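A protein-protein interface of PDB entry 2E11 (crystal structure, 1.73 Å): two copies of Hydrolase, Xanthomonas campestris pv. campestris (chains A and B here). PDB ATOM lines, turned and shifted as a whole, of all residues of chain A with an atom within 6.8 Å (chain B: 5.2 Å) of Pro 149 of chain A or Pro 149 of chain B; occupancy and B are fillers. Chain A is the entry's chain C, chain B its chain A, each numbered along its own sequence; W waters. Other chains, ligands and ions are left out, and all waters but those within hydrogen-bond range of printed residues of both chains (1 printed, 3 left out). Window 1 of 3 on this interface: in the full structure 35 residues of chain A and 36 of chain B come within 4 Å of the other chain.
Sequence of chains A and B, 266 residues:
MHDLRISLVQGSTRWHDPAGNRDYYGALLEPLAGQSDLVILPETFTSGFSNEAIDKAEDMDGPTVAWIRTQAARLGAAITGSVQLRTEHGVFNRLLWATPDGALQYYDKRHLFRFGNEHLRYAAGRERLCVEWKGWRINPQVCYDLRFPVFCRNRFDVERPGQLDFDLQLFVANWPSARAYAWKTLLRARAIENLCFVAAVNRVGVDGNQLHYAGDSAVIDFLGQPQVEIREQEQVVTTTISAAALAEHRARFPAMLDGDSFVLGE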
ATOM      1  N   ARG A 128     -30.950 -23.464  -4.806  1.00  0.00           N
ATOM      2  CA  ARG A 128     -29.517 -23.483  -5.129  1.00  0.00           C
ATOM      3  C   ARG A 128     -29.150 -24.910  -5.532  1.00  0.00           C
ATOM      4  O   ARG A 128     -29.582 -25.861  -4.878  1.00  0.00           O
ATOM      5  CB  ARG A 128     -28.664 -23.034  -3.947  1.00  0.00           C
ATOM      6  CG  ARG A 128     -27.189 -22.908  -4.315  1.00  0.00           C
ATOM      7  CD  ARG A 128     -26.349 -22.278  -3.226  1.00  0.00           C
ATOM      8  NE  ARG A 128     -26.100 -23.209  -2.113  1.00  0.00           N
ATOM      9  CZ  ARG A 128     -25.339 -22.902  -1.068  1.00  0.00           C
ATOM     10  NH1 ARG A 128     -24.814 -21.686  -0.974  1.00  0.00           N
ATOM     11  NH2 ARG A 128     -25.129 -23.797  -0.107  1.00  0.00           N
ATOM     12  N   ASP A 145     -25.431 -13.597  -9.884  1.00  0.00           N
ATOM     13  CA  ASP A 145     -25.407 -14.361  -8.615  1.00  0.00           C
ATOM     14  C   ASP A 145     -24.155 -14.076  -7.787  1.00  0.00           C
ATOM     15  O   ASP A 145     -24.189 -14.101  -6.558  1.00  0.00           O
ATOM     16  CB  ASP A 145     -25.468 -15.870  -8.876  1.00  0.00           C
ATOM     17  CG  ASP A 145     -26.849 -16.359  -9.343  1.00  0.00           C
ATOM     18  OD1 ASP A 145     -27.888 -15.706  -9.070  1.00  0.00           O
ATOM     19  OD2 ASP A 145     -26.886 -17.461  -9.945  1.00  0.00           O
ATOM     20  N   LEU A 146     -23.046 -13.852  -8.477  1.00  0.00           N
ATOM     21  CA  LEU A 146     -21.755 -13.601  -7.826  1.00  0.00           C
ATOM     22  C   LEU A 146     -21.809 -12.445  -6.801  1.00  0.00           C
ATOM     23  O   LEU A 146     -21.055 -12.444  -5.829  1.00  0.00           O
ATOM     24  CB  LEU A 146     -20.711 -13.294  -8.889  1.00  0.00           C
ATOM     25  CG  LEU A 146     -19.271 -12.992  -8.431  1.00  0.00           C
ATOM     26  CD1 LEU A 146     -18.696 -14.156  -7.648  1.00  0.00           C
ATOM     27  CD2 LEU A 146     -18.387 -12.703  -9.626  1.00  0.00           C
ATOM     28  N   ARG A 147     -22.714 -11.487  -7.004  1.00  0.00           N
ATOM     29  CA  ARG A 147     -22.802 -10.315  -6.131  1.00  0.00           C
ATOM     30  C   ARG A 147     -23.570 -10.540  -4.816  1.00  0.00           C
ATOM     31  O   ARG A 147     -23.814  -9.595  -4.057  1.00  0.00           O
ATOM     32  CB  ARG A 147     -23.416  -9.140  -6.914  1.00  0.00           C
ATOM     33  CG  ARG A 147     -22.516  -8.646  -8.029  1.00  0.00           C
ATOM     34  CD  ARG A 147     -23.202  -7.431  -8.693  1.00  0.00           C
ATOM     35  NE  ARG A 147     -22.416  -6.864  -9.794  1.00  0.00           N
ATOM     36  CZ  ARG A 147     -21.541  -5.867  -9.636  1.00  0.00           C
ATOM     37  NH1 ARG A 147     -21.326  -5.367  -8.425  1.00  0.00           N
ATOM     38  NH2 ARG A 147     -20.885  -5.365 -10.681  1.00  0.00           N
ATOM     39  N   PHE A 148     -23.937 -11.797  -4.554  1.00  0.00           N
ATOM     40  CA  PHE A 148     -24.870 -12.126  -3.481  1.00  0.00           C
ATOM     41  C   PHE A 148     -24.288 -13.161  -2.543  1.00  0.00           C
ATOM     42  O   PHE A 148     -24.507 -14.338  -2.716  1.00  0.00           O
ATOM     43  CB  PHE A 148     -26.199 -12.558  -4.107  1.00  0.00           C
ATOM     44  CG  PHE A 148     -26.830 -11.436  -4.886  1.00  0.00           C
ATOM     45  CD1 PHE A 148     -26.560 -11.279  -6.244  1.00  0.00           C
ATOM     46  CD2 PHE A 148     -27.565 -10.457  -4.231  1.00  0.00           C
ATOM     47  CE1 PHE A 148     -27.068 -10.193  -6.939  1.00  0.00           C
ATOM     48  CE2 PHE A 148     -28.097  -9.384  -4.921  1.00  0.00           C
ATOM     49  CZ  PHE A 148     -27.848  -9.246  -6.273  1.00  0.00           C
ATOM     50  N   PRO A 149     -23.504 -12.700  -1.558  1.00  0.00           N
ATOM     51  CA  PRO A 149     -22.711 -13.618  -0.755  1.00  0.00           C
ATOM     52  C   PRO A 149     -23.512 -14.555   0.124  1.00  0.00           C
ATOM     53  O   PRO A 149     -23.027 -15.634   0.429  1.00  0.00           O
ATOM     54  CB  PRO A 149     -21.841 -12.670   0.100  1.00  0.00           C
ATOM     55  CG  PRO A 149     -22.652 -11.430   0.193  1.00  0.00           C
ATOM     56  CD  PRO A 149     -23.269 -11.296  -1.176  1.00  0.00           C
ATOM     57  N   VAL A 150     -24.718 -14.173   0.520  1.00  0.00           N
ATOM     58  CA  VAL A 150     -25.515 -15.065   1.384  1.00  0.00           C
ATOM     59  C   VAL A 150     -25.994 -16.275   0.588  1.00  0.00           C
ATOM     60  O   VAL A 150     -25.862 -17.413   1.043  1.00  0.00           O
ATOM     61  CB  VAL A 150     -26.692 -14.347   2.053  1.00  0.00           C
ATOM     62  CG1 VAL A 150     -27.427 -15.323   2.985  1.00  0.00           C
ATOM     63  CG2 VAL A 150     -26.178 -13.140   2.843  1.00  0.00           C
ATOM     64  N   PHE A 151     -26.478 -16.033  -0.627  1.00  0.00           N
ATOM     65  CA  PHE A 151     -26.871 -17.139  -1.500  1.00  0.00           C
ATOM     66  C   PHE A 151     -25.661 -17.971  -1.947  1.00  0.00           C
ATOM     67  O   PHE A 151     -25.797 -19.151  -2.207  1.00  0.00           O
ATOM     68  CB  PHE A 151     -27.653 -16.635  -2.696  1.00  0.00           C
ATOM     69  CG  PHE A 151     -28.441 -17.717  -3.393  1.00  0.00           C
ATOM     70  CD1 PHE A 151     -28.025 -18.218  -4.625  1.00  0.00           C
ATOM     71  CD2 PHE A 151     -29.595 -18.229  -2.794  1.00  0.00           C
ATOM     72  CE1 PHE A 151     -28.767 -19.235  -5.276  1.00  0.00           C
ATOM     73  CE2 PHE A 151     -30.347 -19.248  -3.421  1.00  0.00           C
ATOM     74  CZ  PHE A 151     -29.928 -19.749  -4.666  1.00  0.00           C
ATOM     75  N   CYS A 152     -24.485 -17.341  -2.009  1.00  0.00           N
ATOM     76  CA  CYS A 152     -23.230 -18.017  -2.376  1.00  0.00           C
ATOM     77  C   CYS A 152     -22.563 -18.752  -1.213  1.00  0.00           C
ATOM     78  O   CYS A 152     -21.558 -19.456  -1.402  1.00  0.00           O
ATOM     79  CB  CYS A 152     -22.213 -17.016  -2.942  1.00  0.00           C
ATOM     80  SG  CYS A 152     -22.609 -16.427  -4.579  1.00  0.00           S
ATOM     81  N   ARG A 153     -23.119 -18.614  -0.014  1.00  0.00           N
ATOM     82  CA  ARG A 153     -22.390 -19.053   1.188  1.00  0.00           C
ATOM     83  C   ARG A 153     -22.200 -20.563   1.320  1.00  0.00           C
ATOM     84  O   ARG A 153     -23.158 -21.331   1.181  1.00  0.00           O
ATOM     85  CB  ARG A 153     -23.056 -18.498   2.449  1.00  0.00           C
ATOM     86  CG  ARG A 153     -22.156 -18.546   3.665  1.00  0.00           C
ATOM     87  CD  ARG A 153     -20.993 -17.579   3.557  1.00  0.00           C
ATOM     88  NE  ARG A 153     -20.314 -17.479   4.845  1.00  0.00           N
ATOM     89  CZ  ARG A 153     -19.203 -18.124   5.173  1.00  0.00           C
ATOM     90  NH1 ARG A 153     -18.732 -17.969   6.398  1.00  0.00           N
ATOM     91  NH2 ARG A 153     -18.568 -18.928   4.296  1.00  0.00           N
ATOM     92  N   ASN A 154     -20.948 -20.956   1.567  1.00  0.00           N
ATOM     93  CA  ASN A 154     -20.562 -22.338   1.871  1.00  0.00           C
ATOM     94  C   ASN A 154     -20.771 -22.566   3.372  1.00  0.00           C
ATOM     95  O   ASN A 154     -19.947 -22.158   4.210  1.00  0.00           O
ATOM     96  CB  ASN A 154     -19.063 -22.531   1.502  1.00  0.00           C
ATOM     97  CG  ASN A 154     -18.694 -23.969   1.148  1.00  0.00           C
ATOM     98  OD1 ASN A 154     -17.528 -24.265   0.826  1.00  0.00           O
ATOM     99  ND2 ASN A 154     -19.654 -24.860   1.212  1.00  0.00           N
ATOM    100  N   ARG A 190     -14.967 -14.861  -2.954  1.00  0.00           N
ATOM    101  CA  ARG A 190     -15.774 -16.069  -2.722  1.00  0.00           C
ATOM    102  C   ARG A 190     -14.903 -17.285  -2.393  1.00  0.00           C
ATOM    103  O   ARG A 190     -15.212 -18.052  -1.467  1.00  0.00           O
ATOM    104  CB  ARG A 190     -16.683 -16.378  -3.928  1.00  0.00           C
ATOM    105  CG  ARG A 190     -17.755 -15.283  -4.181  1.00  0.00           C
ATOM    106  CD  ARG A 190     -18.891 -15.225  -3.151  1.00  0.00           C
ATOM    107  NE  ARG A 190     -19.692 -14.023  -3.424  1.00  0.00           N
ATOM    108  CZ  ARG A 190     -19.518 -12.849  -2.834  1.00  0.00           C
ATOM    109  NH1 ARG A 190     -18.646 -12.726  -1.831  1.00  0.00           N
ATOM    110  NH2 ARG A 190     -20.271 -11.803  -3.191  1.00  0.00           N
ATOM    111  N   GLU A 193     -13.540 -16.676   1.294  1.00  0.00           N
ATOM    112  CA  GLU A 193     -14.489 -16.743   2.398  1.00  0.00           C
ATOM    113  C   GLU A 193     -15.130 -18.116   2.473  1.00  0.00           C
ATOM    114  O   GLU A 193     -15.493 -18.569   3.556  1.00  0.00           O
ATOM    115  CB  GLU A 193     -15.564 -15.659   2.286  1.00  0.00           C
ATOM    116  CG  GLU A 193     -16.516 -15.821   1.118  1.00  0.00           C
ATOM    117  CD  GLU A 193     -17.275 -14.536   0.797  1.00  0.00           C
ATOM    118  OE1 GLU A 193     -18.266 -14.603   0.039  1.00  0.00           O
ATOM    119  OE2 GLU A 193     -16.870 -13.464   1.296  1.00  0.00           O
ATOM    120  N   ASN A 194     -15.279 -18.769   1.323  1.00  0.00           N
ATOM    121  CA  ASN A 194     -15.943 -20.066   1.295  1.00  0.00           C
ATOM    122  C   ASN A 194     -14.967 -21.241   1.344  1.00  0.00           C
ATOM    123  O   ASN A 194     -15.397 -22.398   1.229  1.00  0.00           O
ATOM    124  CB  ASN A 194     -16.844 -20.171   0.071  1.00  0.00           C
ATOM    125  CG  ASN A 194     -18.108 -19.358   0.217  1.00  0.00           C
ATOM    126  OD1 ASN A 194     -18.638 -19.227   1.311  1.00  0.00           O
ATOM    127  ND2 ASN A 194     -18.632 -18.861  -0.894  1.00  0.00           N
ATOM    128  N   ASP A 260     -21.649 -18.420  10.618  1.00  0.00           N
ATOM    129  CA  ASP A 260     -22.915 -18.185  11.315  1.00  0.00           C
ATOM    130  C   ASP A 260     -24.052 -18.986  10.718  1.00  0.00           C
ATOM    131  O   ASP A 260     -24.130 -19.143   9.504  1.00  0.00           O
ATOM    132  CB  ASP A 260     -23.267 -16.698  11.255  1.00  0.00           C
ATOM    133  CG  ASP A 260     -22.227 -15.844  11.939  1.00  0.00           C
ATOM    134  OD1 ASP A 260     -22.117 -15.939  13.187  1.00  0.00           O
ATOM    135  OD2 ASP A 260     -21.493 -15.127  11.225  1.00  0.00           O
ATOM    136  N   PHE A 262     -27.841 -19.427   9.566  1.00  0.00           N
ATOM    137  CA  PHE A 262     -28.889 -18.546   9.076  1.00  0.00           C
ATOM    138  C   PHE A 262     -29.896 -19.350   8.283  1.00  0.00           C
ATOM    139  O   PHE A 262     -29.601 -20.472   7.872  1.00  0.00           O
ATOM    140  CB  PHE A 262     -28.316 -17.415   8.209  1.00  0.00           C
ATOM    141  CG  PHE A 262     -27.655 -17.891   6.948  1.00  0.00           C
ATOM    142  CD1 PHE A 262     -28.384 -17.979   5.754  1.00  0.00           C
ATOM    143  CD2 PHE A 262     -26.318 -18.243   6.940  1.00  0.00           C
ATOM    144  CE1 PHE A 262     -27.772 -18.424   4.568  1.00  0.00           C
ATOM    145  CE2 PHE A 262     -25.699 -18.701   5.757  1.00  0.00           C
ATOM    146  CZ  PHE A 262     -26.416 -18.777   4.578  1.00  0.00           C
ATOM    147  N   LEU B 146     -14.253  -9.839   9.254  1.00  0.00           N
ATOM    148  CA  LEU B 146     -14.211  -9.618   7.802  1.00  0.00           C
ATOM    149  C   LEU B 146     -14.516 -10.869   6.952  1.00  0.00           C
ATOM    150  O   LEU B 146     -15.029 -10.772   5.832  1.00  0.00           O
ATOM    151  CB  LEU B 146     -12.847  -9.023   7.434  1.00  0.00           C
ATOM    152  CG  LEU B 146     -12.548  -8.666   5.971  1.00  0.00           C
ATOM    153  CD1 LEU B 146     -13.592  -7.732   5.374  1.00  0.00           C
ATOM    154  CD2 LEU B 146     -11.158  -8.056   5.891  1.00  0.00           C
ATOM    155  N   ARG B 147     -14.169 -12.043   7.479  1.00  0.00           N
ATOM    156  CA  ARG B 147     -14.258 -13.284   6.693  1.00  0.00           C
ATOM    157  C   ARG B 147     -15.661 -13.852   6.679  1.00  0.00           C
ATOM    158  O   ARG B 147     -15.869 -14.960   6.170  1.00  0.00           O
ATOM    159  CB  ARG B 147     -13.300 -14.333   7.274  1.00  0.00           C
ATOM    160  CG  ARG B 147     -11.829 -13.983   7.030  1.00  0.00           C
ATOM    161  CD  ARG B 147     -10.958 -15.120   7.530  1.00  0.00           C
ATOM    162  NE  ARG B 147      -9.524 -14.870   7.326  1.00  0.00           N
ATOM    163  CZ  ARG B 147      -8.841 -15.279   6.257  1.00  0.00           C
ATOM    164  NH1 ARG B 147      -9.463 -15.968   5.300  1.00  0.00           N
ATOM    165  NH2 ARG B 147      -7.524 -15.031   6.155  1.00  0.00           N
ATOM    166  N   PHE B 148     -16.605 -13.129   7.285  1.00  0.00           N
ATOM    167  CA  PHE B 148     -17.967 -13.657   7.485  1.00  0.00           C
ATOM    168  C   PHE B 148     -19.010 -12.783   6.833  1.00  0.00           C
ATOM    169  O   PHE B 148     -19.553 -11.876   7.463  1.00  0.00           O
ATOM    170  CB  PHE B 148     -18.246 -13.913   8.971  1.00  0.00           C
ATOM    171  CG  PHE B 148     -17.274 -14.862   9.552  1.00  0.00           C
ATOM    172  CD1 PHE B 148     -16.091 -14.388  10.114  1.00  0.00           C
ATOM    173  CD2 PHE B 148     -17.469 -16.248   9.422  1.00  0.00           C
ATOM    174  CE1 PHE B 148     -15.134 -15.271  10.591  1.00  0.00           C
ATOM    175  CE2 PHE B 148     -16.514 -17.136   9.904  1.00  0.00           C
ATOM    176  CZ  PHE B 148     -15.346 -16.644  10.478  1.00  0.00           C
ATOM    177  N   PRO B 149     -19.245 -13.022   5.533  1.00  0.00           N
ATOM    178  CA  PRO B 149     -20.052 -12.116   4.733  1.00  0.00           C
ATOM    179  C   PRO B 149     -21.510 -12.005   5.193  1.00  0.00           C
ATOM    180  O   PRO B 149     -22.136 -10.956   4.991  1.00  0.00           O
ATOM    181  CB  PRO B 149     -19.954 -12.735   3.319  1.00  0.00           C
ATOM    182  CG  PRO B 149     -19.713 -14.172   3.580  1.00  0.00           C
ATOM    183  CD  PRO B 149     -18.745 -14.148   4.729  1.00  0.00           C
ATOM    184  N   VAL B 150     -22.044 -13.067   5.794  1.00  0.00           N
ATOM    185  CA  VAL B 150     -23.453 -13.041   6.195  1.00  0.00           C
ATOM    186  C   VAL B 150     -23.631 -12.052   7.348  1.00  0.00           C
ATOM    187  O   VAL B 150     -24.518 -11.209   7.312  1.00  0.00           O
ATOM    188  CB  VAL B 150     -23.995 -14.447   6.539  1.00  0.00           C
ATOM    189  CG1 VAL B 150     -25.432 -14.317   7.034  1.00  0.00           C
ATOM    190  CG2 VAL B 150     -23.913 -15.357   5.283  1.00  0.00           C
ATOM    191  N   PHE B 151     -22.760 -12.132   8.342  1.00  0.00           N
ATOM    192  CA  PHE B 151     -22.799 -11.161   9.426  1.00  0.00           C
ATOM    193  C   PHE B 151     -22.435  -9.737   8.974  1.00  0.00           C
ATOM    194  O   PHE B 151     -22.942  -8.753   9.531  1.00  0.00           O
ATOM    195  CB  PHE B 151     -21.913 -11.641  10.585  1.00  0.00           C
ATOM    196  CG  PHE B 151     -22.150 -10.901  11.852  1.00  0.00           C
ATOM    197  CD1 PHE B 151     -21.225  -9.970  12.316  1.00  0.00           C
ATOM    198  CD2 PHE B 151     -23.318 -11.103  12.582  1.00  0.00           C
ATOM    199  CE1 PHE B 151     -21.453  -9.263  13.507  1.00  0.00           C
ATOM    200  CE2 PHE B 151     -23.558 -10.390  13.784  1.00  0.00           C
ATOM    201  CZ  PHE B 151     -22.625  -9.474  14.238  1.00  0.00           C
ATOM    202  N   CYS B 152     -21.587  -9.615   7.953  1.00  0.00           N
ATOM    203  CA  CYS B 152     -21.255  -8.292   7.390  1.00  0.00           C
ATOM    204  C   CYS B 152     -22.343  -7.731   6.472  1.00  0.00           C
ATOM    205  O   CYS B 152     -22.201  -6.622   5.982  1.00  0.00           O
ATOM    206  CB  CYS B 152     -19.971  -8.362   6.559  1.00  0.00           C
ATOM    207  SG  CYS B 152     -18.487  -8.613   7.552  1.00  0.00           S
ATOM    208  N   ARG B 153     -23.408  -8.490   6.207  1.00  0.00           N
ATOM    209  CA  ARG B 153     -24.235  -8.152   5.038  1.00  0.00           C
ATOM    210  C   ARG B 153     -25.050  -6.877   5.256  1.00  0.00           C
ATOM    211  O   ARG B 153     -25.669  -6.712   6.312  1.00  0.00           O
ATOM    212  CB  ARG B 153     -25.180  -9.310   4.644  1.00  0.00           C
ATOM    213  CG  ARG B 153     -25.822  -9.095   3.287  1.00  0.00           C
ATOM    214  CD  ARG B 153     -24.843  -9.349   2.135  1.00  0.00           C
ATOM    215  NE  ARG B 153     -25.561  -9.436   0.861  1.00  0.00           N
ATOM    216  CZ  ARG B 153     -25.818  -8.419   0.034  1.00  0.00           C
ATOM    217  NH1 ARG B 153     -25.382  -7.189   0.292  1.00  0.00           N
ATOM    218  NH2 ARG B 153     -26.515  -8.645  -1.074  1.00  0.00           N
ATOM    219  N   ARG B 190     -16.266  -6.543   0.194  1.00  0.00           N
ATOM    220  CA  ARG B 190     -17.345  -6.076   1.071  1.00  0.00           C
ATOM    221  C   ARG B 190     -17.925  -4.777   0.538  1.00  0.00           C
ATOM    222  O   ARG B 190     -19.136  -4.615   0.492  1.00  0.00           O
ATOM    223  CB  ARG B 190     -16.895  -5.900   2.523  1.00  0.00           C
ATOM    224  CG  ARG B 190     -16.502  -7.210   3.232  1.00  0.00           C
ATOM    225  CD  ARG B 190     -17.663  -8.159   3.515  1.00  0.00           C
ATOM    226  NE  ARG B 190     -17.100  -9.459   3.903  1.00  0.00           N
ATOM    227  CZ  ARG B 190     -16.972 -10.510   3.111  1.00  0.00           C
ATOM    228  NH1 ARG B 190     -17.419 -10.480   1.848  1.00  0.00           N
ATOM    229  NH2 ARG B 190     -16.402 -11.625   3.578  1.00  0.00           N
ATOM    230  N   GLU B 193     -20.067  -5.641  -2.740  1.00  0.00           N
ATOM    231  CA  GLU B 193     -21.299  -6.411  -2.571  1.00  0.00           C
ATOM    232  C   GLU B 193     -22.285  -5.653  -1.673  1.00  0.00           C
ATOM    233  O   GLU B 193     -23.503  -5.783  -1.848  1.00  0.00           O
ATOM    234  CB  GLU B 193     -21.022  -7.826  -2.051  1.00  0.00           C
ATOM    235  CG  GLU B 193     -20.634  -7.881  -0.606  1.00  0.00           C
ATOM    236  CD  GLU B 193     -19.867  -9.141  -0.222  1.00  0.00           C
ATOM    237  OE1 GLU B 193     -19.638  -9.293   0.990  1.00  0.00           O
ATOM    238  OE2 GLU B 193     -19.486  -9.959  -1.107  1.00  0.00           O
HETATM  239  O   HOH W   1     -24.502  -6.942  -4.031  1.00  0.00           O
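The side-chain carboxylate of Glu 193 of chain A lies within salt-bridge range of the guanidinium group of Arg 190 of chain B (3.0 Å).
The side-chain carboxylate (OE2) of Glu 193 of chain B lies within salt-bridge range of the guanidinium group (NH2) of Arg 190 of chain A.
The guanidinium group (NH2) of Arg 190 of chain B sits at hydrogen-bond distance from the backbone carbonyl oxygen (O) of Leu 146 of chain B, 2.8 Å away.
The guanidinium group (NH1) of Arg 190 of chain B is in salt-bridge range of the side-chain carboxylate (OE1) of Glu 193 of chain B (2.7 Å).
O of Arg 153 of chain A sits at hydrogen-bond distance from NH1 of Arg 128 of chain A, 2.7 Å away.
The side-chain sulfur of Cys 152 of chain A lies within hydrogen-bond range of the backbone carbonyl oxygen of Phe 148 of chain A, 3.4 Å away.
The guanidinium group (NH2) of Arg 153 of chain A lies within hydrogen-bond range of the side-chain amide oxygen (OD1) of Asn 194 of chain A.
The side-chain carboxylate of Glu 193 of chain A lies within salt-bridge range of the guanidinium group of Arg 190 of chain A, 2.7 Å away.
Among the printed residues, merely in contact across the chains: Asp 260 of chain A with Phe 151 of chain B, Pro 149 of chain A with Arg 153 of chain B, Arg 153 of chain A with Pro 149 of chain B, Pro 149 of chain A with Glu 193 of chain B, Arg 153 of chain A with Phe 148 of chain B, Glu 193 of chain A with Pro 149 of chain B, Pro 149 of chain A with Pro 149 of chain B, Phe 148 of chain A with Arg 153 of chain B, Phe 262 of chain A with Val 150 of chain B, Arg 147 of chain A with Glu 193 of chain B, Glu 193 of chain A with Arg 147 of chain B, Arg 153 of chain A with Val 150 of chain B and Val 150 of chain A with Val 150 of chain B.
Pro 149 of chain A touches three residues of chain B.
Printed residues of chain B within 4 Å of Asp 260 of chain A: Phe 151.
Of the printed residues of chain A, Val 150 of chain B touches Val 150 (3.9999 Å), Arg 153 (3.98 Å) and Phe 262 (3.8 Å).
Printed residues of chain A within 4 Å of Arg 153 of chain B: Phe 148 (3.8 Å) and Pro 149 (3.6 Å).
The nearest residue of chain B that does not touch Pro 149 of chain A is Val 150 of chain B (4.9 Å).
The nearest printed residue of chain A that does not touch Arg 153 of chain B is Val 150 of chain A (4.1 Å).
Printed residues of chain A that touch a printed residue of chain B: Arg 147, Phe 148, Pro 149, Val 150, Arg 153, Arg 190, Glu 193, Asp 260 and Phe 262.
Of the 10 printed residues of chain B, 8 touch a printed residue of chain A.
Along chain B the printed residues that touch a printed residue of chain A span positions 147 to 193.
Among the printed residues, 15 pairs touch across the chains.
Phe 148 of chain A touches Arg 153 of chain B, and with the chains exchanged Arg 153 of chain A touches Phe 148 of chain B.
Pro 149 of chain B touches its own counterpart, Pro 149 of chain A.
Pro 149 of chain A touches Arg 153 of chain B, and with the chains exchanged Arg 153 of chain A touches Pro 149 of chain B.
Val 150 of chain B touches its own counterpart, Val 150 of chain A.
Of the 15 pairs that touch across the chains among the printed residues, 12 have their exchanged pair printed and touching as well.
Water W1 bridges O of Glu 193 of chain B and O of Arg 147 of chain A.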
